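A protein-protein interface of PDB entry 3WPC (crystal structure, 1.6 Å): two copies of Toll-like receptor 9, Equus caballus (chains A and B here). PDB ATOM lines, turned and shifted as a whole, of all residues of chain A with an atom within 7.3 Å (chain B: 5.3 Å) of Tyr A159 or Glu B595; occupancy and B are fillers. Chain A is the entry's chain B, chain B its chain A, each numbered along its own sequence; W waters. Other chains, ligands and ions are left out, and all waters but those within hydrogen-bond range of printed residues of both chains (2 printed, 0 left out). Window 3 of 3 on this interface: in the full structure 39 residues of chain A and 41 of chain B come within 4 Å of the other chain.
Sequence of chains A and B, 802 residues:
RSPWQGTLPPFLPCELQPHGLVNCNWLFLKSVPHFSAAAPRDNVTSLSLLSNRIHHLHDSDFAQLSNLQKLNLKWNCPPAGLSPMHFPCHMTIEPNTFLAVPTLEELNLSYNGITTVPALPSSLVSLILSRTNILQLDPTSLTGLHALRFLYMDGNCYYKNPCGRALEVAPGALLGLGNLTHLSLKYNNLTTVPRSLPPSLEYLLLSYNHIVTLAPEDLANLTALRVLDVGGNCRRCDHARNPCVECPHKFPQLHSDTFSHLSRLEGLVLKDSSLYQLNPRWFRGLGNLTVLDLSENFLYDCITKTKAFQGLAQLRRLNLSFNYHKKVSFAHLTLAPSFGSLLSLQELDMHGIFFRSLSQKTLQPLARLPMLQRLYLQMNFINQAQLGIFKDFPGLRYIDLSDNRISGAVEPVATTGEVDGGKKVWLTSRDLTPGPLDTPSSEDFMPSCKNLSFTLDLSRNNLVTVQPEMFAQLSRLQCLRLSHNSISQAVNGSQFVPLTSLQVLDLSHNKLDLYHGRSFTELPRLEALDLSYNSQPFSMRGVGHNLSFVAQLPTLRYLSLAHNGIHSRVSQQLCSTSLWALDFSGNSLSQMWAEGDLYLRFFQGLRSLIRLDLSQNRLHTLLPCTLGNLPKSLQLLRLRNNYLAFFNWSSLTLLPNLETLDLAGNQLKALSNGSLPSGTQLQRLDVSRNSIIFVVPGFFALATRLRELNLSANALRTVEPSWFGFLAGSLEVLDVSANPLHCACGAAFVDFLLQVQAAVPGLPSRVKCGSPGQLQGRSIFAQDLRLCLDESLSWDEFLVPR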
ATOM      1  N   GLY A  81      16.718  -7.203 -16.316  1.00  0.00           N
ATOM      2  CA  GLY A  81      18.074  -7.159 -15.767  1.00  0.00           C
ATOM      3  C   GLY A  81      18.697  -5.811 -15.554  1.00  0.00           C
ATOM      4  O   GLY A  81      19.571  -5.645 -14.690  1.00  0.00           O
ATOM      5  N   LEU A  82      18.293  -4.847 -16.388  1.00  0.00           N
ATOM      6  CA  LEU A  82      18.758  -3.486 -16.351  1.00  0.00           C
ATOM      7  C   LEU A  82      17.859  -2.505 -15.583  1.00  0.00           C
ATOM      8  O   LEU A  82      18.318  -1.470 -15.164  1.00  0.00           O
ATOM      9  CB  LEU A  82      18.962  -3.010 -17.788  1.00  0.00           C
ATOM     10  CG  LEU A  82      20.005  -3.893 -18.493  1.00  0.00           C
ATOM     11  CD1 LEU A  82      19.859  -3.820 -19.993  1.00  0.00           C
ATOM     12  CD2 LEU A  82      21.363  -3.452 -18.053  1.00  0.00           C
ATOM     13  N   CYS A 157      22.984  -9.991 -24.525  1.00  0.00           N
ATOM     14  CA  CYS A 157      23.040 -11.297 -23.819  1.00  0.00           C
ATOM     15  C   CYS A 157      24.289 -11.376 -22.993  1.00  0.00           C
ATOM     16  O   CYS A 157      25.329 -11.870 -23.469  1.00  0.00           O
ATOM     17  CB  CYS A 157      23.000 -12.461 -24.817  1.00  0.00           C
ATOM     18  SG  CYS A 157      22.704 -14.029 -23.944  1.00  0.00           S
ATOM     19  N   TYR A 158      24.189 -10.925 -21.738  1.00  0.00           N
ATOM     20  CA  TYR A 158      25.272 -11.005 -20.794  1.00  0.00           C
ATOM     21  C   TYR A 158      24.701 -10.946 -19.389  1.00  0.00           C
ATOM     22  O   TYR A 158      23.477 -10.987 -19.237  1.00  0.00           O
ATOM     23  CB  TYR A 158      26.239  -9.838 -21.035  1.00  0.00           C
ATOM     24  CG  TYR A 158      25.804  -8.431 -20.637  1.00  0.00           C
ATOM     25  CD1 TYR A 158      24.755  -7.781 -21.287  1.00  0.00           C
ATOM     26  CD2 TYR A 158      26.547  -7.679 -19.694  1.00  0.00           C
ATOM     27  CE1 TYR A 158      24.396  -6.498 -20.966  1.00  0.00           C
ATOM     28  CE2 TYR A 158      26.198  -6.367 -19.401  1.00  0.00           C
ATOM     29  CZ  TYR A 158      25.127  -5.776 -20.022  1.00  0.00           C
ATOM     30  OH  TYR A 158      24.800  -4.484 -19.690  1.00  0.00           O
ATOM     31  N   TYR A 159      25.558 -10.835 -18.368  1.00  0.00           N
ATOM     32  CA  TYR A 159      25.060 -11.051 -16.995  1.00  0.00           C
ATOM     33  C   TYR A 159      23.971 -10.072 -16.518  1.00  0.00           C
ATOM     34  O   TYR A 159      23.101 -10.469 -15.742  1.00  0.00           O
ATOM     35  CB  TYR A 159      26.203 -11.101 -15.972  1.00  0.00           C
ATOM     36  CG  TYR A 159      26.911  -9.797 -15.759  1.00  0.00           C
ATOM     37  CD1 TYR A 159      27.832  -9.346 -16.674  1.00  0.00           C
ATOM     38  CD2 TYR A 159      26.674  -9.012 -14.648  1.00  0.00           C
ATOM     39  CE1 TYR A 159      28.473  -8.138 -16.518  1.00  0.00           C
ATOM     40  CE2 TYR A 159      27.360  -7.828 -14.446  1.00  0.00           C
ATOM     41  CZ  TYR A 159      28.241  -7.385 -15.445  1.00  0.00           C
ATOM     42  OH  TYR A 159      28.995  -6.263 -15.262  1.00  0.00           O
ATOM     43  N   LYS A 160      24.009  -8.817 -16.981  1.00  0.00           N
ATOM     44  CA  LYS A 160      22.968  -7.836 -16.672  1.00  0.00           C
ATOM     45  C   LYS A 160      21.696  -7.931 -17.552  1.00  0.00           C
ATOM     46  O   LYS A 160      20.726  -7.222 -17.344  1.00  0.00           O
ATOM     47  CB  LYS A 160      23.538  -6.422 -16.774  1.00  0.00           C
ATOM     48  CG  LYS A 160      24.615  -6.094 -15.786  1.00  0.00           C
ATOM     49  CD  LYS A 160      24.792  -4.596 -15.536  1.00  0.00           C
ATOM     50  CE  LYS A 160      25.799  -4.361 -14.410  1.00  0.00           C
ATOM     51  NZ  LYS A 160      26.305  -2.971 -14.346  1.00  0.00           N
ATOM     52  N   ASN A 161      21.718  -8.796 -18.568  1.00  0.00           N
ATOM     53  CA  ASN A 161      20.601  -8.922 -19.498  1.00  0.00           C
ATOM     54  C   ASN A 161      20.680 -10.289 -20.140  1.00  0.00           C
ATOM     55  O   ASN A 161      21.043 -10.406 -21.350  1.00  0.00           O
ATOM     56  CB  ASN A 161      20.688  -7.774 -20.552  1.00  0.00           C
ATOM     57  CG  ASN A 161      19.541  -7.751 -21.530  1.00  0.00           C
ATOM     58  OD1 ASN A 161      18.412  -8.047 -21.181  1.00  0.00           O
ATOM     59  ND2 ASN A 161      19.801  -7.272 -22.757  1.00  0.00           N
ATOM     60  N   PRO A 162      20.423 -11.349 -19.347  1.00  0.00           N
ATOM     61  CA  PRO A 162      20.729 -12.692 -19.822  1.00  0.00           C
ATOM     62  C   PRO A 162      19.719 -13.197 -20.841  1.00  0.00           C
ATOM     63  O   PRO A 162      18.592 -12.679 -20.900  1.00  0.00           O
ATOM     64  CB  PRO A 162      20.760 -13.525 -18.536  1.00  0.00           C
ATOM     65  CG  PRO A 162      19.928 -12.803 -17.579  1.00  0.00           C
ATOM     66  CD  PRO A 162      20.080 -11.335 -17.911  1.00  0.00           C
ATOM     67  N   CYS A 163      20.128 -14.174 -21.658  1.00  0.00           N
ATOM     68  CA  CYS A 163      19.256 -14.724 -22.661  1.00  0.00           C
ATOM     69  C   CYS A 163      19.263 -16.242 -22.840  1.00  0.00           C
ATOM     70  O   CYS A 163      18.361 -16.760 -23.516  1.00  0.00           O
ATOM     71  CB  CYS A 163      19.563 -14.057 -24.013  1.00  0.00           C
ATOM     72  SG  CYS A 163      20.973 -14.750 -24.885  1.00  0.00           S
ATOM     73  N   TYR A 187      29.307  -7.952 -25.726  1.00  0.00           N
ATOM     74  CA  TYR A 187      28.401  -8.435 -24.655  1.00  0.00           C
ATOM     75  C   TYR A 187      27.133  -9.158 -25.165  1.00  0.00           C
ATOM     76  O   TYR A 187      26.013  -8.954 -24.682  1.00  0.00           O
ATOM     77  CB  TYR A 187      28.009  -7.274 -23.726  1.00  0.00           C
ATOM     78  CG  TYR A 187      29.154  -6.607 -22.927  1.00  0.00           C
ATOM     79  CD1 TYR A 187      29.670  -7.208 -21.795  1.00  0.00           C
ATOM     80  CD2 TYR A 187      29.683  -5.403 -23.306  1.00  0.00           C
ATOM     81  CE1 TYR A 187      30.667  -6.615 -21.054  1.00  0.00           C
ATOM     82  CE2 TYR A 187      30.660  -4.793 -22.550  1.00  0.00           C
ATOM     83  CZ  TYR A 187      31.172  -5.430 -21.466  1.00  0.00           C
ATOM     84  OH  TYR A 187      32.188  -4.971 -20.671  1.00  0.00           O
ATOM     85  N   ARG A 235      38.932 -13.997 -20.544  1.00  0.00           N
ATOM     86  CA  ARG A 235      39.311 -13.098 -19.462  1.00  0.00           C
ATOM     87  C   ARG A 235      40.158 -13.665 -18.348  1.00  0.00           C
ATOM     88  O   ARG A 235      40.128 -14.857 -18.085  1.00  0.00           O
ATOM     89  CB  ARG A 235      38.045 -12.483 -18.862  1.00  0.00           C
ATOM     90  CG  ARG A 235      37.189 -11.734 -19.835  1.00  0.00           C
ATOM     91  CD  ARG A 235      36.026 -11.022 -19.185  1.00  0.00           C
ATOM     92  NE  ARG A 235      36.492  -9.967 -18.281  1.00  0.00           N
ATOM     93  CZ  ARG A 235      35.751  -9.457 -17.288  1.00  0.00           C
ATOM     94  NH1 ARG A 235      34.521  -9.915 -17.040  1.00  0.00           N
ATOM     95  NH2 ARG A 235      36.267  -8.538 -16.486  1.00  0.00           N
ATOM     96  N   ARG A 241      36.324  -6.915 -12.055  1.00  0.00           N
ATOM     97  CA  ARG A 241      35.498  -6.240 -11.040  1.00  0.00           C
ATOM     98  C   ARG A 241      34.052  -6.696 -11.099  1.00  0.00           C
ATOM     99  O   ARG A 241      33.288  -6.381 -10.229  1.00  0.00           O
ATOM    100  CB  ARG A 241      35.620  -4.715 -11.099  1.00  0.00           C
ATOM    101  CG  ARG A 241      34.973  -4.077 -12.290  1.00  0.00           C
ATOM    102  CD  ARG A 241      34.760  -2.570 -12.109  1.00  0.00           C
ATOM    103  NE  ARG A 241      33.775  -2.158 -13.098  1.00  0.00           N
ATOM    104  CZ  ARG A 241      33.505  -0.909 -13.446  1.00  0.00           C
ATOM    105  NH1 ARG A 241      34.155   0.101 -12.880  1.00  0.00           N
ATOM    106  NH2 ARG A 241      32.581  -0.675 -14.389  1.00  0.00           N
ATOM    107  N   ASN A 242      33.697  -7.462 -12.132  1.00  0.00           N
ATOM    108  CA  ASN A 242      32.344  -7.882 -12.388  1.00  0.00           C
ATOM    109  C   ASN A 242      32.305  -9.410 -12.516  1.00  0.00           C
ATOM    110  O   ASN A 242      33.350 -10.093 -12.438  1.00  0.00           O
ATOM    111  CB  ASN A 242      31.795  -7.181 -13.642  1.00  0.00           C
ATOM    112  CG  ASN A 242      32.588  -7.469 -14.904  1.00  0.00           C
ATOM    113  OD1 ASN A 242      33.689  -7.969 -14.872  1.00  0.00           O
ATOM    114  ND2 ASN A 242      31.984  -7.165 -16.039  1.00  0.00           N
ATOM    115  N   PRO A 243      31.078  -9.970 -12.634  1.00  0.00           N
ATOM    116  CA  PRO A 243      30.973 -11.419 -12.881  1.00  0.00           C
ATOM    117  C   PRO A 243      31.784 -11.810 -14.101  1.00  0.00           C
ATOM    118  O   PRO A 243      31.813 -11.082 -15.104  1.00  0.00           O
ATOM    119  CB  PRO A 243      29.464 -11.626 -13.114  1.00  0.00           C
ATOM    120  CG  PRO A 243      28.826 -10.497 -12.331  1.00  0.00           C
ATOM    121  CD  PRO A 243      29.738  -9.324 -12.596  1.00  0.00           C
ATOM    122  N   CYS A 244      32.468 -12.935 -13.984  1.00  0.00           N
ATOM    123  CA  CYS A 244      33.467 -13.288 -14.963  1.00  0.00           C
ATOM    124  C   CYS A 244      33.460 -14.805 -15.151  1.00  0.00           C
ATOM    125  O   CYS A 244      33.451 -15.566 -14.185  1.00  0.00           O
ATOM    126  CB  CYS A 244      34.811 -12.730 -14.476  1.00  0.00           C
ATOM    127  SG  CYS A 244      36.178 -12.926 -15.628  1.00  0.00           S
ATOM    128  N   GLN B 591      27.733   1.465  -6.029  1.00  0.00           N
ATOM    129  CA  GLN B 591      28.458   0.787  -7.106  1.00  0.00           C
ATOM    130  C   GLN B 591      28.461  -0.729  -6.926  1.00  0.00           C
ATOM    131  O   GLN B 591      28.229  -1.493  -7.877  1.00  0.00           O
ATOM    132  CB  GLN B 591      29.885   1.357  -7.254  1.00  0.00           C
ATOM    133  CG  GLN B 591      30.707   0.624  -8.293  1.00  0.00           C
ATOM    134  CD  GLN B 591      31.939   1.402  -8.730  1.00  0.00           C
ATOM    135  OE1 GLN B 591      32.198   2.532  -8.255  1.00  0.00           O
ATOM    136  NE2 GLN B 591      32.705   0.810  -9.662  1.00  0.00           N
ATOM    137  N   MET B 592      28.672  -1.181  -5.681  1.00  0.00           N
ATOM    138  CA  MET B 592      28.757  -2.584  -5.385  1.00  0.00           C
ATOM    139  C   MET B 592      27.428  -3.285  -5.705  1.00  0.00           C
ATOM    140  O   MET B 592      27.409  -4.327  -6.370  1.00  0.00           O
ATOM    141  CB  MET B 592      29.121  -2.759  -3.894  1.00  0.00           C
ATOM    142  CG  MET B 592      30.531  -2.307  -3.584  1.00  0.00           C
ATOM    143  SD  MET B 592      30.862  -2.185  -1.826  1.00  0.00           S
ATOM    144  CE  MET B 592      30.592  -3.847  -1.226  1.00  0.00           C
ATOM    145  N   TRP B 593      26.322  -2.678  -5.314  1.00  0.00           N
ATOM    146  CA  TRP B 593      25.046  -3.321  -5.489  1.00  0.00           C
ATOM    147  C   TRP B 593      24.535  -3.186  -6.918  1.00  0.00           C
ATOM    148  O   TRP B 593      23.599  -3.874  -7.318  1.00  0.00           O
ATOM    149  CB  TRP B 593      24.025  -2.832  -4.444  1.00  0.00           C
ATOM    150  CG  TRP B 593      24.150  -3.484  -3.083  1.00  0.00           C
ATOM    151  CD1 TRP B 593      24.805  -4.626  -2.792  1.00  0.00           C
ATOM    152  CD2 TRP B 593      23.564  -3.020  -1.874  1.00  0.00           C
ATOM    153  NE1 TRP B 593      24.675  -4.919  -1.465  1.00  0.00           N
ATOM    154  CE2 TRP B 593      23.899  -3.954  -0.869  1.00  0.00           C
ATOM    155  CE3 TRP B 593      22.752  -1.937  -1.540  1.00  0.00           C
ATOM    156  CZ2 TRP B 593      23.464  -3.817   0.449  1.00  0.00           C
ATOM    157  CZ3 TRP B 593      22.326  -1.791  -0.221  1.00  0.00           C
ATOM    158  CH2 TRP B 593      22.685  -2.729   0.751  1.00  0.00           C
ATOM    159  N   ALA B 594      25.153  -2.322  -7.703  1.00  0.00           N
ATOM    160  CA  ALA B 594      24.849  -2.332  -9.160  1.00  0.00           C
ATOM    161  C   ALA B 594      25.603  -3.416  -9.934  1.00  0.00           C
ATOM    162  O   ALA B 594      25.339  -3.582 -11.137  1.00  0.00           O
ATOM    163  CB  ALA B 594      25.182  -0.995  -9.755  1.00  0.00           C
ATOM    164  N   GLU B 595      26.586  -4.059  -9.298  1.00  0.00           N
ATOM    165  CA  GLU B 595      27.494  -4.988  -9.959  1.00  0.00           C
ATOM    166  C   GLU B 595      26.966  -6.456 -10.065  1.00  0.00           C
ATOM    167  O   GLU B 595      27.505  -7.404  -9.477  1.00  0.00           O
ATOM    168  CB  GLU B 595      28.883  -4.934  -9.305  1.00  0.00           C
ATOM    169  CG  GLU B 595      29.956  -5.600 -10.126  1.00  0.00           C
ATOM    170  CD  GLU B 595      29.934  -5.204 -11.582  1.00  0.00           C
ATOM    171  OE1 GLU B 595      30.668  -4.247 -11.898  1.00  0.00           O
ATOM    172  OE2 GLU B 595      29.187  -5.834 -12.407  1.00  0.00           O
ATOM    173  N   GLY B 596      25.891  -6.626 -10.827  1.00  0.00           N
ATOM    174  CA  GLY B 596      25.220  -7.896 -10.867  1.00  0.00           C
ATOM    175  C   GLY B 596      24.947  -8.414  -9.455  1.00  0.00           C
ATOM    176  O   GLY B 596      24.589  -7.637  -8.550  1.00  0.00           O
ATOM    177  N   ASP B 597      25.152  -9.698  -9.268  1.00  0.00           N
ATOM    178  CA  ASP B 597      24.811 -10.333  -7.999  1.00  0.00           C
ATOM    179  C   ASP B 597      25.999 -10.426  -7.034  1.00  0.00           C
ATOM    180  O   ASP B 597      25.902 -11.042  -5.956  1.00  0.00           O
ATOM    181  CB  ASP B 597      24.198 -11.731  -8.237  1.00  0.00           C
ATOM    182  CG  ASP B 597      25.175 -12.752  -8.822  1.00  0.00           C
ATOM    183  OD1 ASP B 597      26.401 -12.517  -8.961  1.00  0.00           O
ATOM    184  OD2 ASP B 597      24.681 -13.855  -9.159  1.00  0.00           O
ATOM    185  N   LEU B 598      27.128  -9.813  -7.384  1.00  0.00           N
ATOM    186  CA  LEU B 598      28.389 -10.080  -6.685  1.00  0.00           C
ATOM    187  C   LEU B 598      28.321  -9.758  -5.196  1.00  0.00           C
ATOM    188  O   LEU B 598      28.835 -10.524  -4.375  1.00  0.00           O
ATOM    189  CB  LEU B 598      29.567  -9.288  -7.275  1.00  0.00           C
ATOM    190  CG  LEU B 598      30.155  -9.771  -8.597  1.00  0.00           C
ATOM    191  CD1 LEU B 598      31.406  -8.955  -8.921  1.00  0.00           C
ATOM    192  CD2 LEU B 598      30.465 -11.269  -8.564  1.00  0.00           C
ATOM    193  N   TYR B 599      27.706  -8.632  -4.869  1.00  0.00           N
ATOM    194  CA  TYR B 599      27.767  -8.098  -3.524  1.00  0.00           C
ATOM    195  C   TYR B 599      26.393  -8.096  -2.827  1.00  0.00           C
ATOM    196  O   TYR B 599      26.239  -7.463  -1.806  1.00  0.00           O
ATOM    197  CB  TYR B 599      28.350  -6.658  -3.537  1.00  0.00           C
ATOM    198  CG  TYR B 599      29.753  -6.579  -4.074  1.00  0.00           C
ATOM    199  CD1 TYR B 599      30.803  -7.025  -3.352  1.00  0.00           C
ATOM    200  CD2 TYR B 599      30.022  -6.063  -5.362  1.00  0.00           C
ATOM    201  CE1 TYR B 599      32.097  -6.997  -3.804  1.00  0.00           C
ATOM    202  CE2 TYR B 599      31.326  -5.984  -5.811  1.00  0.00           C
ATOM    203  CZ  TYR B 599      32.354  -6.478  -5.074  1.00  0.00           C
ATOM    204  OH  TYR B 599      33.648  -6.367  -5.551  1.00  0.00           O
HETATM  205  O   HOH W   1      28.795  -2.566 -12.777  1.00  0.00           O
HETATM  206  O   HOH W   2      33.798  -5.108  -7.925  1.00  0.00           O
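The side-chain carboxylate (OE2) of Glu B595 lies within hydrogen-bond range of the side-chain hydroxyl (OH) of Tyr A159 (2.9 Å).
The side-chain amino group of Lys A160 sits close to the backbone carbonyl oxygen of Ala B594, at 3.4 Å.
OE1 of Glu B595 is in salt-bridge range of NE of Arg A241.
The guanidinium group (NH1) of Arg A235 sits at hydrogen-bond distance from the side-chain amide oxygen (OD1) of Asn A242, at 3.0 Å.
The side-chain hydroxyl (OH) of Tyr A159 sits at hydrogen-bond distance from the side-chain amide nitrogen (ND2) of Asn A242, 3.2 Å away.
The side-chain sulfur (SG) of Cys A157 forms a disulfide with the side-chain sulfur (SG) of Cys A163.
Among the printed residues, merely in contact across the chains: Arg A241 with Gln B591, Arg A241 with Leu B598, Asn A242 with Glu B595, Asn A242 with Leu B598, Pro A243 with Glu B595 and Pro A243 with Leu B598.
Tyr A159 touches just one residue of chain B: Glu B595 (2.9 Å).
Of chain A, only Tyr A159 (2.9 Å), Arg A241 (3.4 Å), Asn A242 (3.2 Å) and Pro A243 (3.5 Å) come within 4 Å of Glu B595.
No residue of chain A comes within 4 Å of Gly B596.
Printed residues of chain B within 4 Å of Pro A243: Glu B595 (3.5 Å) and Leu B598 (3.9 Å).
Of the printed residues of chain B, Lys A160 touches Ala B594 (3.4 Å).
Of the printed residues of chain A, Ala B594 touches Lys A160 (3.4 Å).
Tyr A158 touches none of the printed residues of chain B.
The nearest residue of chain B that does not touch Tyr A159 is Gly B596 (4.1 Å).
The nearest residue of chain A that does not touch Glu B595 is Lys A160 (4.2 Å).
Of the 9 printed residues of chain B, 4 touch a printed residue of chain A.
Hydrophobic or aromatic side chains of chain B that line the printed part of chain A: Leu B598.
Hydrophobic or aromatic side chains of chain A within 4 Å of the printed part of chain B: Tyr A159 and Pro A243.
Among the printed residues, 9 pairs touch across the chains.
Among the printed residues, Asp or Glu carboxylates within 4 Å of a Lys or Arg side-chain nitrogen of the other chain: Arg A241 with Glu B595.
No position is printed for both chains.
Water W1 lies within hydrogen-bond range of the side-chain carboxylate (OE1) of Glu B595 (2.7 Å) and the side-chain amino group (NZ) of Lys A160 (3.0 Å).
Water W2 lies within hydrogen-bond range of O of Arg A241 (2.7 Å) and OH of Tyr B599 (2.7 Å).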
